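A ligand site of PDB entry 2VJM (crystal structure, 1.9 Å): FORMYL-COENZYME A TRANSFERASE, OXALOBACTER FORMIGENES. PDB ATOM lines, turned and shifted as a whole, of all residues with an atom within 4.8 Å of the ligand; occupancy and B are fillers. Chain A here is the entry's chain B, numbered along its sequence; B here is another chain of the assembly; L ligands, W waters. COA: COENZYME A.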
ATOM      1  N   HIS A  15       9.455   9.165 -30.641  1.00  0.00           N
ATOM      2  CA  HIS A  15       9.811   9.438 -32.031  1.00  0.00           C
ATOM      3  C   HIS A  15      10.274   8.152 -32.700  1.00  0.00           C
ATOM      4  O   HIS A  15      10.499   7.142 -32.039  1.00  0.00           O
ATOM      5  CB  HIS A  15      10.886  10.543 -32.121  1.00  0.00           C
ATOM      6  CG  HIS A  15      12.215  10.160 -31.555  1.00  0.00           C
ATOM      7  ND1 HIS A  15      13.386  10.757 -31.972  1.00  0.00           N
ATOM      8  CD2 HIS A  15      12.578   9.241 -30.619  1.00  0.00           C
ATOM      9  CE1 HIS A  15      14.404  10.240 -31.307  1.00  0.00           C
ATOM     10  NE2 HIS A  15      13.940   9.316 -30.485  1.00  0.00           N
ATOM     11  N   VAL A  16      10.388   8.197 -34.022  1.00  0.00           N
ATOM     12  CA  VAL A  16      10.733   7.026 -34.846  1.00  0.00           C
ATOM     13  C   VAL A  16       9.593   5.970 -34.806  1.00  0.00           C
ATOM     14  O   VAL A  16       8.465   6.310 -35.157  1.00  0.00           O
ATOM     15  CB  VAL A  16      12.138   6.456 -34.525  1.00  0.00           C
ATOM     16  CG1 VAL A  16      12.628   5.547 -35.660  1.00  0.00           C
ATOM     17  CG2 VAL A  16      13.152   7.599 -34.303  1.00  0.00           C
ATOM     18  N   GLN A  17       9.855   4.734 -34.357  1.00  0.00           N
ATOM     19  CA  GLN A  17       8.856   3.661 -34.505  1.00  0.00           C
ATOM     20  C   GLN A  17       8.389   3.002 -33.203  1.00  0.00           C
ATOM     21  O   GLN A  17       7.187   2.920 -32.979  1.00  0.00           O
ATOM     22  CB  GLN A  17       9.328   2.584 -35.475  1.00  0.00           C
ATOM     23  CG  GLN A  17       8.245   1.524 -35.722  1.00  0.00           C
ATOM     24  CD  GLN A  17       8.602   0.408 -36.695  1.00  0.00           C
ATOM     25  OE1 GLN A  17       8.013  -0.667 -36.647  1.00  0.00           O
ATOM     26  NE2 GLN A  17       9.561   0.660 -37.581  1.00  0.00           N
ATOM     27  N   ALA A  18       9.317   2.516 -32.373  1.00  0.00           N
ATOM     28  CA  ALA A  18       8.946   1.752 -31.175  1.00  0.00           C
ATOM     29  C   ALA A  18       8.021   2.515 -30.223  1.00  0.00           C
ATOM     30  O   ALA A  18       6.931   2.047 -29.890  1.00  0.00           O
ATOM     31  CB  ALA A  18      10.198   1.271 -30.427  1.00  0.00           C
ATOM     32  N   GLU A  37       7.036  17.482 -29.989  1.00  0.00           N
ATOM     33  CA  GLU A  37       7.950  17.396 -31.130  1.00  0.00           C
ATOM     34  C   GLU A  37       8.987  18.514 -31.162  1.00  0.00           C
ATOM     35  O   GLU A  37       8.753  19.611 -30.677  1.00  0.00           O
ATOM     36  CB  GLU A  37       7.170  17.385 -32.443  1.00  0.00           C
ATOM     37  CG  GLU A  37       6.172  16.252 -32.514  1.00  0.00           C
ATOM     38  CD  GLU A  37       5.624  16.034 -33.893  1.00  0.00           C
ATOM     39  OE1 GLU A  37       6.420  15.728 -34.818  1.00  0.00           O
ATOM     40  OE2 GLU A  37       4.398  16.147 -34.050  1.00  0.00           O
ATOM     41  N   ARG A  38      10.112  18.190 -31.791  1.00  0.00           N
ATOM     42  CA  ARG A  38      11.185  19.146 -32.048  1.00  0.00           C
ATOM     43  C   ARG A  38      10.649  20.285 -32.936  1.00  0.00           C
ATOM     44  O   ARG A  38       9.968  20.034 -33.925  1.00  0.00           O
ATOM     45  CB  ARG A  38      12.344  18.423 -32.738  1.00  0.00           C
ATOM     46  CG  ARG A  38      13.713  18.931 -32.361  1.00  0.00           C
ATOM     47  CD  ARG A  38      14.803  18.268 -33.195  1.00  0.00           C
ATOM     48  NE  ARG A  38      15.257  16.976 -32.656  1.00  0.00           N
ATOM     49  CZ  ARG A  38      16.142  16.831 -31.670  1.00  0.00           C
ATOM     50  NH1 ARG A  38      16.664  17.882 -31.051  1.00  0.00           N
ATOM     51  NH2 ARG A  38      16.496  15.608 -31.281  1.00  0.00           N
ATOM     52  N   LEU A  72       7.958  22.003 -29.110  1.00  0.00           N
ATOM     53  CA  LEU A  72       8.515  22.466 -27.835  1.00  0.00           C
ATOM     54  C   LEU A  72      10.038  22.343 -27.804  1.00  0.00           C
ATOM     55  O   LEU A  72      10.579  21.264 -28.090  1.00  0.00           O
ATOM     56  CB  LEU A  72       7.917  21.664 -26.672  1.00  0.00           C
ATOM     57  CG  LEU A  72       8.193  22.173 -25.259  1.00  0.00           C
ATOM     58  CD1 LEU A  72       7.608  23.587 -25.063  1.00  0.00           C
ATOM     59  CD2 LEU A  72       7.619  21.215 -24.225  1.00  0.00           C
ATOM     60  N   ASP A  73      10.722  23.432 -27.472  1.00  0.00           N
ATOM     61  CA  ASP A  73      12.152  23.365 -27.192  1.00  0.00           C
ATOM     62  C   ASP A  73      12.300  23.090 -25.695  1.00  0.00           C
ATOM     63  O   ASP A  73      12.086  23.981 -24.873  1.00  0.00           O
ATOM     64  CB  ASP A  73      12.890  24.646 -27.608  1.00  0.00           C
ATOM     65  CG  ASP A  73      14.407  24.506 -27.532  1.00  0.00           C
ATOM     66  OD1 ASP A  73      14.904  23.560 -26.864  1.00  0.00           O
ATOM     67  OD2 ASP A  73      15.114  25.342 -28.133  1.00  0.00           O
ATOM     68  N   MET A  74      12.635  21.849 -25.368  1.00  0.00           N
ATOM     69  CA  MET A  74      12.721  21.402 -23.982  1.00  0.00           C
ATOM     70  C   MET A  74      14.037  21.798 -23.298  1.00  0.00           C
ATOM     71  O   MET A  74      14.179  21.580 -22.094  1.00  0.00           O
ATOM     72  CB  MET A  74      12.516  19.878 -23.910  1.00  0.00           C
ATOM     73  CG  MET A  74      11.151  19.427 -24.441  1.00  0.00           C
ATOM     74  SD  MET A  74      10.849  17.663 -24.272  1.00  0.00           S
ATOM     75  CE  MET A  74      11.885  17.014 -25.572  1.00  0.00           C
ATOM     76  N   LYS A  75      14.970  22.374 -24.049  1.00  0.00           N
ATOM     77  CA  LYS A  75      16.218  22.873 -23.448  1.00  0.00           C
ATOM     78  C   LYS A  75      16.062  24.292 -22.891  1.00  0.00           C
ATOM     79  O   LYS A  75      16.954  24.786 -22.190  1.00  0.00           O
ATOM     80  CB  LYS A  75      17.390  22.838 -24.452  1.00  0.00           C
ATOM     81  CG  LYS A  75      17.434  21.599 -25.341  1.00  0.00           C
ATOM     82  CD  LYS A  75      18.850  21.083 -25.607  1.00  0.00           C
ATOM     83  CE  LYS A  75      19.228  19.951 -24.661  1.00  0.00           C
ATOM     84  NZ  LYS A  75      20.387  19.150 -25.170  1.00  0.00           N
ATOM     85  N   ASN A  96      11.299   7.468 -25.857  1.00  0.00           N
ATOM     86  CA  ASN A  96      12.339   6.598 -26.378  1.00  0.00           C
ATOM     87  C   ASN A  96      13.497   7.426 -26.931  1.00  0.00           C
ATOM     88  O   ASN A  96      13.944   7.229 -28.063  1.00  0.00           O
ATOM     89  CB  ASN A  96      11.778   5.579 -27.392  1.00  0.00           C
ATOM     90  CG  ASN A  96      11.247   6.215 -28.674  1.00  0.00           C
ATOM     91  OD1 ASN A  96      10.544   7.232 -28.646  1.00  0.00           O
ATOM     92  ND2 ASN A  96      11.541   5.584 -29.816  1.00  0.00           N
ATOM     93  N   PHE A  97      13.973   8.360 -26.111  1.00  0.00           N
ATOM     94  CA  PHE A  97      15.218   9.065 -26.365  1.00  0.00           C
ATOM     95  C   PHE A  97      16.394   8.136 -26.048  1.00  0.00           C
ATOM     96  O   PHE A  97      16.219   7.066 -25.478  1.00  0.00           O
ATOM     97  CB  PHE A  97      15.361  10.321 -25.491  1.00  0.00           C
ATOM     98  CG  PHE A  97      14.330  11.406 -25.777  1.00  0.00           C
ATOM     99  CD1 PHE A  97      13.532  11.893 -24.750  1.00  0.00           C
ATOM    100  CD2 PHE A  97      14.195  11.944 -27.044  1.00  0.00           C
ATOM    101  CE1 PHE A  97      12.601  12.908 -24.999  1.00  0.00           C
ATOM    102  CE2 PHE A  97      13.277  12.955 -27.297  1.00  0.00           C
ATOM    103  CZ  PHE A  97      12.473  13.423 -26.270  1.00  0.00           C
ATOM    104  N   GLY A  98      17.599   8.579 -26.411  1.00  0.00           N
ATOM    105  CA  GLY A  98      18.805   7.829 -26.077  1.00  0.00           C
ATOM    106  C   GLY A  98      18.981   7.713 -24.571  1.00  0.00           C
ATOM    107  O   GLY A  98      18.323   8.443 -23.810  1.00  0.00           O
ATOM    108  N   PRO A  99      19.856   6.794 -24.119  1.00  0.00           N
ATOM    109  CA  PRO A  99      20.093   6.584 -22.691  1.00  0.00           C
ATOM    110  C   PRO A  99      20.439   7.890 -21.953  1.00  0.00           C
ATOM    111  O   PRO A  99      21.315   8.638 -22.413  1.00  0.00           O
ATOM    112  CB  PRO A  99      21.277   5.613 -22.654  1.00  0.00           C
ATOM    113  CG  PRO A  99      21.244   4.919 -23.964  1.00  0.00           C
ATOM    114  CD  PRO A  99      20.676   5.887 -24.951  1.00  0.00           C
ATOM    115  N   ALA A 101      18.879  10.693 -21.742  1.00  0.00           N
ATOM    116  CA  ALA A 101      18.460  11.961 -22.361  1.00  0.00           C
ATOM    117  C   ALA A 101      17.415  12.726 -21.534  1.00  0.00           C
ATOM    118  O   ALA A 101      17.602  13.900 -21.230  1.00  0.00           O
ATOM    119  CB  ALA A 101      17.947  11.732 -23.790  1.00  0.00           C
ATOM    120  N   ARG A 104      18.882  14.036 -18.275  1.00  0.00           N
ATOM    121  CA  ARG A 104      19.692  15.237 -18.519  1.00  0.00           C
ATOM    122  C   ARG A 104      18.865  16.505 -18.694  1.00  0.00           C
ATOM    123  O   ARG A 104      19.353  17.608 -18.425  1.00  0.00           O
ATOM    124  CB  ARG A 104      20.615  15.021 -19.723  1.00  0.00           C
ATOM    125  CG  ARG A 104      21.778  14.095 -19.424  1.00  0.00           C
ATOM    126  CD  ARG A 104      22.813  14.099 -20.522  1.00  0.00           C
ATOM    127  NE  ARG A 104      22.315  13.505 -21.758  1.00  0.00           N
ATOM    128  CZ  ARG A 104      22.269  12.196 -22.005  1.00  0.00           C
ATOM    129  NH1 ARG A 104      21.794  11.774 -23.169  1.00  0.00           N
ATOM    130  NH2 ARG A 104      22.690  11.299 -21.123  1.00  0.00           N
ATOM    131  N   MET A 105      17.615  16.346 -19.152  1.00  0.00           N
ATOM    132  CA  MET A 105      16.675  17.461 -19.242  1.00  0.00           C
ATOM    133  C   MET A 105      16.191  17.895 -17.866  1.00  0.00           C
ATOM    134  O   MET A 105      15.546  18.938 -17.736  1.00  0.00           O
ATOM    135  CB  MET A 105      15.471  17.088 -20.125  1.00  0.00           C
ATOM    136  CG  MET A 105      15.705  17.280 -21.615  1.00  0.00           C
ATOM    137  SD  MET A 105      14.387  16.572 -22.640  1.00  0.00           S
ATOM    138  CE  MET A 105      12.939  17.053 -21.711  1.00  0.00           C
ATOM    139  N   VAL A 124      11.262   3.073 -23.879  1.00  0.00           N
ATOM    140  CA  VAL A 124      11.929   2.077 -24.713  1.00  0.00           C
ATOM    141  C   VAL A 124      13.421   2.382 -24.680  1.00  0.00           C
ATOM    142  O   VAL A 124      13.819   3.531 -24.877  1.00  0.00           O
ATOM    143  CB  VAL A 124      11.456   2.074 -26.184  1.00  0.00           C
ATOM    144  CG1 VAL A 124      12.218   1.019 -26.985  1.00  0.00           C
ATOM    145  CG2 VAL A 124       9.951   1.835 -26.268  1.00  0.00           C
ATOM    146  N   LYS A 125      14.223   1.354 -24.412  1.00  0.00           N
ATOM    147  CA  LYS A 125      15.683   1.458 -24.450  1.00  0.00           C
ATOM    148  C   LYS A 125      16.222   0.372 -25.375  1.00  0.00           C
ATOM    149  O   LYS A 125      15.506  -0.570 -25.702  1.00  0.00           O
ATOM    150  CB  LYS A 125      16.269   1.289 -23.042  1.00  0.00           C
ATOM    151  CG  LYS A 125      15.555   2.047 -21.897  1.00  0.00           C
ATOM    152  CD  LYS A 125      15.947   1.433 -20.540  1.00  0.00           C
ATOM    153  CE  LYS A 125      15.386   2.168 -19.319  1.00  0.00           C
ATOM    154  NZ  LYS A 125      15.779   3.619 -19.233  1.00  0.00           N
ATOM    155  N   GLY A 126      17.471   0.497 -25.797  1.00  0.00           N
ATOM    156  CA  GLY A 126      18.130  -0.527 -26.608  1.00  0.00           C
ATOM    157  C   GLY A 126      18.448  -1.770 -25.784  1.00  0.00           C
ATOM    158  O   GLY A 126      18.063  -2.886 -26.147  1.00  0.00           O
ATOM    159  N   LYS A 137      23.054   3.304 -28.363  1.00  0.00           N
ATOM    160  CA  LYS A 137      21.913   3.656 -29.193  1.00  0.00           C
ATOM    161  C   LYS A 137      21.628   2.503 -30.164  1.00  0.00           C
ATOM    162  O   LYS A 137      22.557   1.915 -30.741  1.00  0.00           O
ATOM    163  CB  LYS A 137      22.165   4.980 -29.927  1.00  0.00           C
ATOM    164  CG  LYS A 137      22.207   6.194 -28.993  1.00  0.00           C
ATOM    165  CD  LYS A 137      22.461   7.508 -29.736  1.00  0.00           C
ATOM    166  CE  LYS A 137      22.385   8.705 -28.788  1.00  0.00           C
ATOM    167  NZ  LYS A 137      22.649  10.006 -29.512  1.00  0.00           N
ATOM    168  N   VAL A 138      20.358   2.159 -30.331  1.00  0.00           N
ATOM    169  CA  VAL A 138      19.949   0.936 -31.035  1.00  0.00           C
ATOM    170  C   VAL A 138      18.804   1.243 -31.994  1.00  0.00           C
ATOM    171  O   VAL A 138      17.854   1.926 -31.612  1.00  0.00           O
ATOM    172  CB  VAL A 138      19.542  -0.167 -30.021  1.00  0.00           C
ATOM    173  CG1 VAL A 138      18.920  -1.378 -30.716  1.00  0.00           C
ATOM    174  CG2 VAL A 138      20.730  -0.595 -29.167  1.00  0.00           C
ATOM    175  N   TYR A 139      18.929   0.764 -33.243  1.00  0.00           N
ATOM    176  CA  TYR A 139      17.847   0.780 -34.234  1.00  0.00           C
ATOM    177  C   TYR A 139      17.402  -0.660 -34.481  1.00  0.00           C
ATOM    178  O   TYR A 139      18.134  -1.592 -34.185  1.00  0.00           O
ATOM    179  CB  TYR A 139      18.302   1.369 -35.575  1.00  0.00           C
ATOM    180  CG  TYR A 139      18.279   2.877 -35.687  1.00  0.00           C
ATOM    181  CD1 TYR A 139      17.073   3.587 -35.578  1.00  0.00           C
ATOM    182  CD2 TYR A 139      19.442   3.586 -35.937  1.00  0.00           C
ATOM    183  CE1 TYR A 139      17.044   4.982 -35.696  1.00  0.00           C
ATOM    184  CE2 TYR A 139      19.429   4.987 -36.059  1.00  0.00           C
ATOM    185  CZ  TYR A 139      18.229   5.674 -35.931  1.00  0.00           C
ATOM    186  OH  TYR A 139      18.218   7.053 -36.049  1.00  0.00           O
ATOM    187  N   A0A A 169      11.503  -2.771 -33.261  1.00  0.00           N
ATOM    188  CA  A0A A 169      10.791  -1.486 -33.048  1.00  0.00           C
ATOM    189  C   A0A A 169       9.356  -1.669 -32.570  1.00  0.00           C
ATOM    190  O   A0A A 169       9.087  -1.576 -31.369  1.00  0.00           O
ATOM    191  CB  A0A A 169      10.834  -0.668 -34.345  1.00  0.00           C
ATOM    192  CG  A0A A 169      12.197  -0.180 -34.786  1.00  0.00           C
ATOM    193  OD1 A0A A 169      13.215  -0.353 -34.113  1.00  0.00           O
ATOM    194  OD2 A0A A 169      12.291   0.498 -36.079  1.00  0.00           O
ATOM    195  CM1 A0A A 169      12.909   1.827 -36.067  1.00  0.00           C
ATOM    196  OM2 A0A A 169      14.117   1.949 -35.903  1.00  0.00           O
ATOM    197  N   MET A 200      14.801  -3.193 -26.207  1.00  0.00           N
ATOM    198  CA  MET A 200      14.593  -3.803 -27.514  1.00  0.00           C
ATOM    199  C   MET A 200      15.175  -5.223 -27.599  1.00  0.00           C
ATOM    200  O   MET A 200      14.539  -6.124 -28.164  1.00  0.00           O
ATOM    201  CB  MET A 200      15.155  -2.916 -28.631  1.00  0.00           C
ATOM    202  CG  MET A 200      14.423  -1.561 -28.742  1.00  0.00           C
ATOM    203  SD  MET A 200      15.351  -0.308 -29.645  1.00  0.00           S
ATOM    204  CE  MET A 200      15.250  -0.939 -31.301  1.00  0.00           C
ATOM    205  N   ASN B 287      22.633  11.357 -40.630  1.00  0.00           N
ATOM    206  CA  ASN B 287      23.284  12.405 -39.836  1.00  0.00           C
ATOM    207  C   ASN B 287      24.668  12.004 -39.296  1.00  0.00           C
ATOM    208  O   ASN B 287      25.233  12.703 -38.461  1.00  0.00           O
ATOM    209  CB  ASN B 287      22.383  12.833 -38.669  1.00  0.00           C
ATOM    210  CG  ASN B 287      22.190  11.728 -37.641  1.00  0.00           C
ATOM    211  OD1 ASN B 287      22.114  10.551 -37.981  1.00  0.00           O
ATOM    212  ND2 ASN B 287      22.098  12.114 -36.372  1.00  0.00           N
HETATM  213  N1A COA L   1      13.780  19.806 -27.544  1.00  0.00           N
HETATM  214  C2A COA L   1      15.042  19.849 -26.993  1.00  0.00           C
HETATM  215  N3A COA L   1      15.858  18.726 -27.027  1.00  0.00           N
HETATM  216  C4A COA L   1      15.407  17.571 -27.595  1.00  0.00           C
HETATM  217  C5A COA L   1      14.131  17.511 -28.150  1.00  0.00           C
HETATM  218  C6A COA L   1      13.307  18.637 -28.120  1.00  0.00           C
HETATM  219  N6A COA L   1      12.063  18.622 -28.577  1.00  0.00           N
HETATM  220  N7A COA L   1      13.969  16.262 -28.630  1.00  0.00           N
HETATM  221  C8A COA L   1      15.085  15.536 -28.399  1.00  0.00           C
HETATM  222  N9A COA L   1      15.990  16.337 -27.756  1.00  0.00           N
HETATM  223  C1B COA L   1      17.370  15.996 -27.352  1.00  0.00           C
HETATM  224  C2B COA L   1      17.472  14.767 -26.465  1.00  0.00           C
HETATM  225  O2B COA L   1      17.124  15.003 -25.123  1.00  0.00           O
HETATM  226  C3B COA L   1      18.937  14.417 -26.646  1.00  0.00           C
HETATM  227  O3B COA L   1      19.705  15.202 -25.774  1.00  0.00           O
HETATM  228  P3B COA L   1      21.199  14.839 -25.312  1.00  0.00           P
HETATM  229  O7A COA L   1      21.259  15.143 -23.844  1.00  0.00           O
HETATM  230  O8A COA L   1      21.515  13.380 -25.551  1.00  0.00           O
HETATM  231  O9A COA L   1      22.194  15.679 -26.079  1.00  0.00           O
HETATM  232  C4B COA L   1      19.228  14.812 -28.089  1.00  0.00           C
HETATM  233  O4B COA L   1      18.191  15.708 -28.469  1.00  0.00           O
HETATM  234  C5B COA L   1      19.280  13.631 -29.051  1.00  0.00           C
HETATM  235  O5B COA L   1      18.192  12.763 -28.828  1.00  0.00           O
HETATM  236  P1A COA L   1      18.294  11.198 -29.185  1.00  0.00           P
HETATM  237  O1A COA L   1      17.054  10.485 -28.747  1.00  0.00           O
HETATM  238  O2A COA L   1      19.552  10.563 -28.665  1.00  0.00           O
HETATM  239  O3A COA L   1      18.291  11.238 -30.797  1.00  0.00           O
HETATM  240  P2A COA L   1      19.361  10.504 -31.741  1.00  0.00           P
HETATM  241  O4A COA L   1      20.775  10.852 -31.360  1.00  0.00           O
HETATM  242  O5A COA L   1      19.007  10.885 -33.164  1.00  0.00           O
HETATM  243  O6A COA L   1      19.147   8.924 -31.551  1.00  0.00           O
HETATM  244  CBP COA L   1      17.745   6.980 -31.339  1.00  0.00           C
HETATM  245  CCP COA L   1      17.990   8.296 -32.064  1.00  0.00           C
HETATM  246  CDP COA L   1      18.936   6.060 -31.644  1.00  0.00           C
HETATM  247  CEP COA L   1      16.489   6.348 -31.933  1.00  0.00           C
HETATM  248  CAP COA L   1      17.590   7.224 -29.829  1.00  0.00           C
HETATM  249  OAP COA L   1      16.502   8.101 -29.568  1.00  0.00           O
HETATM  250  C9P COA L   1      17.445   5.931 -29.060  1.00  0.00           C
HETATM  251  O9P COA L   1      18.572   5.118 -28.831  1.00  0.00           O
HETATM  252  N8P COA L   1      16.231   5.597 -28.642  1.00  0.00           N
HETATM  253  C7P COA L   1      16.013   4.454 -27.765  1.00  0.00           C
HETATM  254  C6P COA L   1      15.873   3.148 -28.540  1.00  0.00           C
HETATM  255  C5P COA L   1      14.861   3.348 -29.652  1.00  0.00           C
HETATM  256  O5P COA L   1      13.679   3.585 -29.383  1.00  0.00           O
HETATM  257  N4P COA L   1      15.332   3.277 -30.895  1.00  0.00           N
HETATM  258  C3P COA L   1      14.450   3.522 -32.009  1.00  0.00           C
HETATM  259  C2P COA L   1      13.570   2.326 -32.337  1.00  0.00           C
HETATM  260  S1P COA L   1      12.175   2.853 -33.364  1.00  0.00           S
HETATM  261  O   HOH W   1      19.068  18.743 -28.950  1.00  0.00           O
HETATM  262  O   HOH W   2      11.397  15.935 -29.502  1.00  0.00           O
HETATM  263  O   HOH W   3      22.754  17.184 -22.940  1.00  0.00           O
HETATM  264  O   HOH W   4      20.917  10.830 -26.421  1.00  0.00           O
HETATM  265  O   HOH W   5      18.969   2.940 -27.360  1.00  0.00           O
HETATM  266  O   HOH W   6      18.811  15.840 -22.958  1.00  0.00           O
HETATM  267  O   HOH W   7      23.021  12.194 -27.903  1.00  0.00           O
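NZ of Lys 137 lies within salt-bridge range of O4A of the ligand. The guanidinium group of Arg 104 lies within salt-bridge range of an oxygen (O7A) of the ligand (2.9 Å). The backbone carbonyl oxygen of Asn 96 sits at hydrogen-bond distance from a nitrogen (N8P) of the ligand, 2.9 Å away. An oxygen (O5P) of the ligand lies within hydrogen-bond range of the side-chain amide nitrogen (ND2) of Asn 96, 3.0 Å away. A nitrogen (N4P) of the ligand sits at hydrogen-bond distance from the backbone carbonyl oxygen (O) of Val 138 (2.9 Å). A ring nitrogen (NE2) of His 15 is in hydrogen-bond range of an oxygen (OAP) of the ligand, 3.0 Å away. OM2 of A0A 169 lies close to a sulfur (S1P) of the ligand (3.3 Å). The backbone NH (N) of Ala 18 lies close to a sulfur (S1P) of the ligand (3.0 Å). The backbone NH (N) of Gly 98 sits at hydrogen-bond distance from an oxygen (O1A) of the ligand (3.1 Å). A nitrogen (N6A) of the ligand sits at hydrogen-bond distance from the backbone carbonyl oxygen (O) of Leu 72 (3.1 Å). The backbone NH (N) of Gln 17 sits close to a sulfur (S1P) of the ligand (3.1 Å). The backbone NH of Met 74 is in hydrogen-bond range of a nitrogen (N1A) of the ligand. The guanidinium group (NH2) of Arg 38 lies close to an oxygen (O4B) of the ligand (3.3 Å). A nitrogen (N8P) of the ligand sits close to the backbone carbonyl oxygen (O) of Phe 97, 3.5 Å away. A nitrogen (N4P) of the ligand lies close to the side-chain sulfur of Met 200, at 3.8 Å.
The guanidinium group (NH1) of Arg 104 sits at hydrogen-bond distance from the backbone carbonyl oxygen (O) of Pro 99 (3.3 Å). O of His 15 is in hydrogen-bond range of ND2 of Asn 96. OD2 of A0A 169 lies within hydrogen-bond range of NE2 of Gln 17 (3.1 Å). N of Leu 72 is in hydrogen-bond range of O of Glu 37, 3.0 Å away. The backbone NH (N) of Lys 75 sits at hydrogen-bond distance from the side-chain carboxylate (OD1) of Asp 73, 3.1 Å away. N of Met 200 lies within hydrogen-bond range of O of Gly 126. The backbone NH of Met 200 sits at hydrogen-bond distance from the backbone carbonyl oxygen of Lys 125, 2.8 Å away.
CG1 of Val 16 touches S1P of the ligand (3.6 Å). Asp 73 touches the ligand (OD1 to C2A, 3.7 Å). CG of Lys 75 touches C2A of the ligand (3.4 Å). CB of Ala 101 touches O2B of the ligand, 3.6 Å away. Val 124 touches the ligand (O to C7P, 3.7 Å). Hydrophobic or aromatic side chains that line the ligand: His 15, Val 16, Ala 18, Met 74, Phe 97, Ala 101, Val 124 and Met 200. 19 residues have an atom within 4 Å of the ligand: His 15, Val 16, Gln 17, Ala 18, Arg 38, Leu 72, Asp 73, Met 74, Lys 75, Asn 96, Phe 97, Gly 98, Ala 101, Arg 104, Val 124, Lys 137, Val 138, A0A 169 and Met 200.
Water W4 lies within hydrogen-bond range of an oxygen (O2A) of the ligand (2.6 Å) and the guanidinium group (NH1) of Arg 104 (3.5 Å). Water W5 lies within hydrogen-bond range of O9P of the ligand (2.7 Å), N of Gly 126 (3.3 Å) and N of Val 138 (3.4 Å). Water W6 lies within hydrogen-bond range of O7A of the ligand (2.7 Å) and O of Ala 101 (2.9 Å). Water W2 lies within hydrogen-bond range of N7A of the ligand (2.7 Å) and N of Arg 38 (3.5 Å). Water W7 lies within hydrogen-bond range of NZ of Lys 137 and O8A of the ligand. Water W1 bridges O4B of the ligand (3.2 Å) and NH1 of Arg 38 (3.3 Å).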
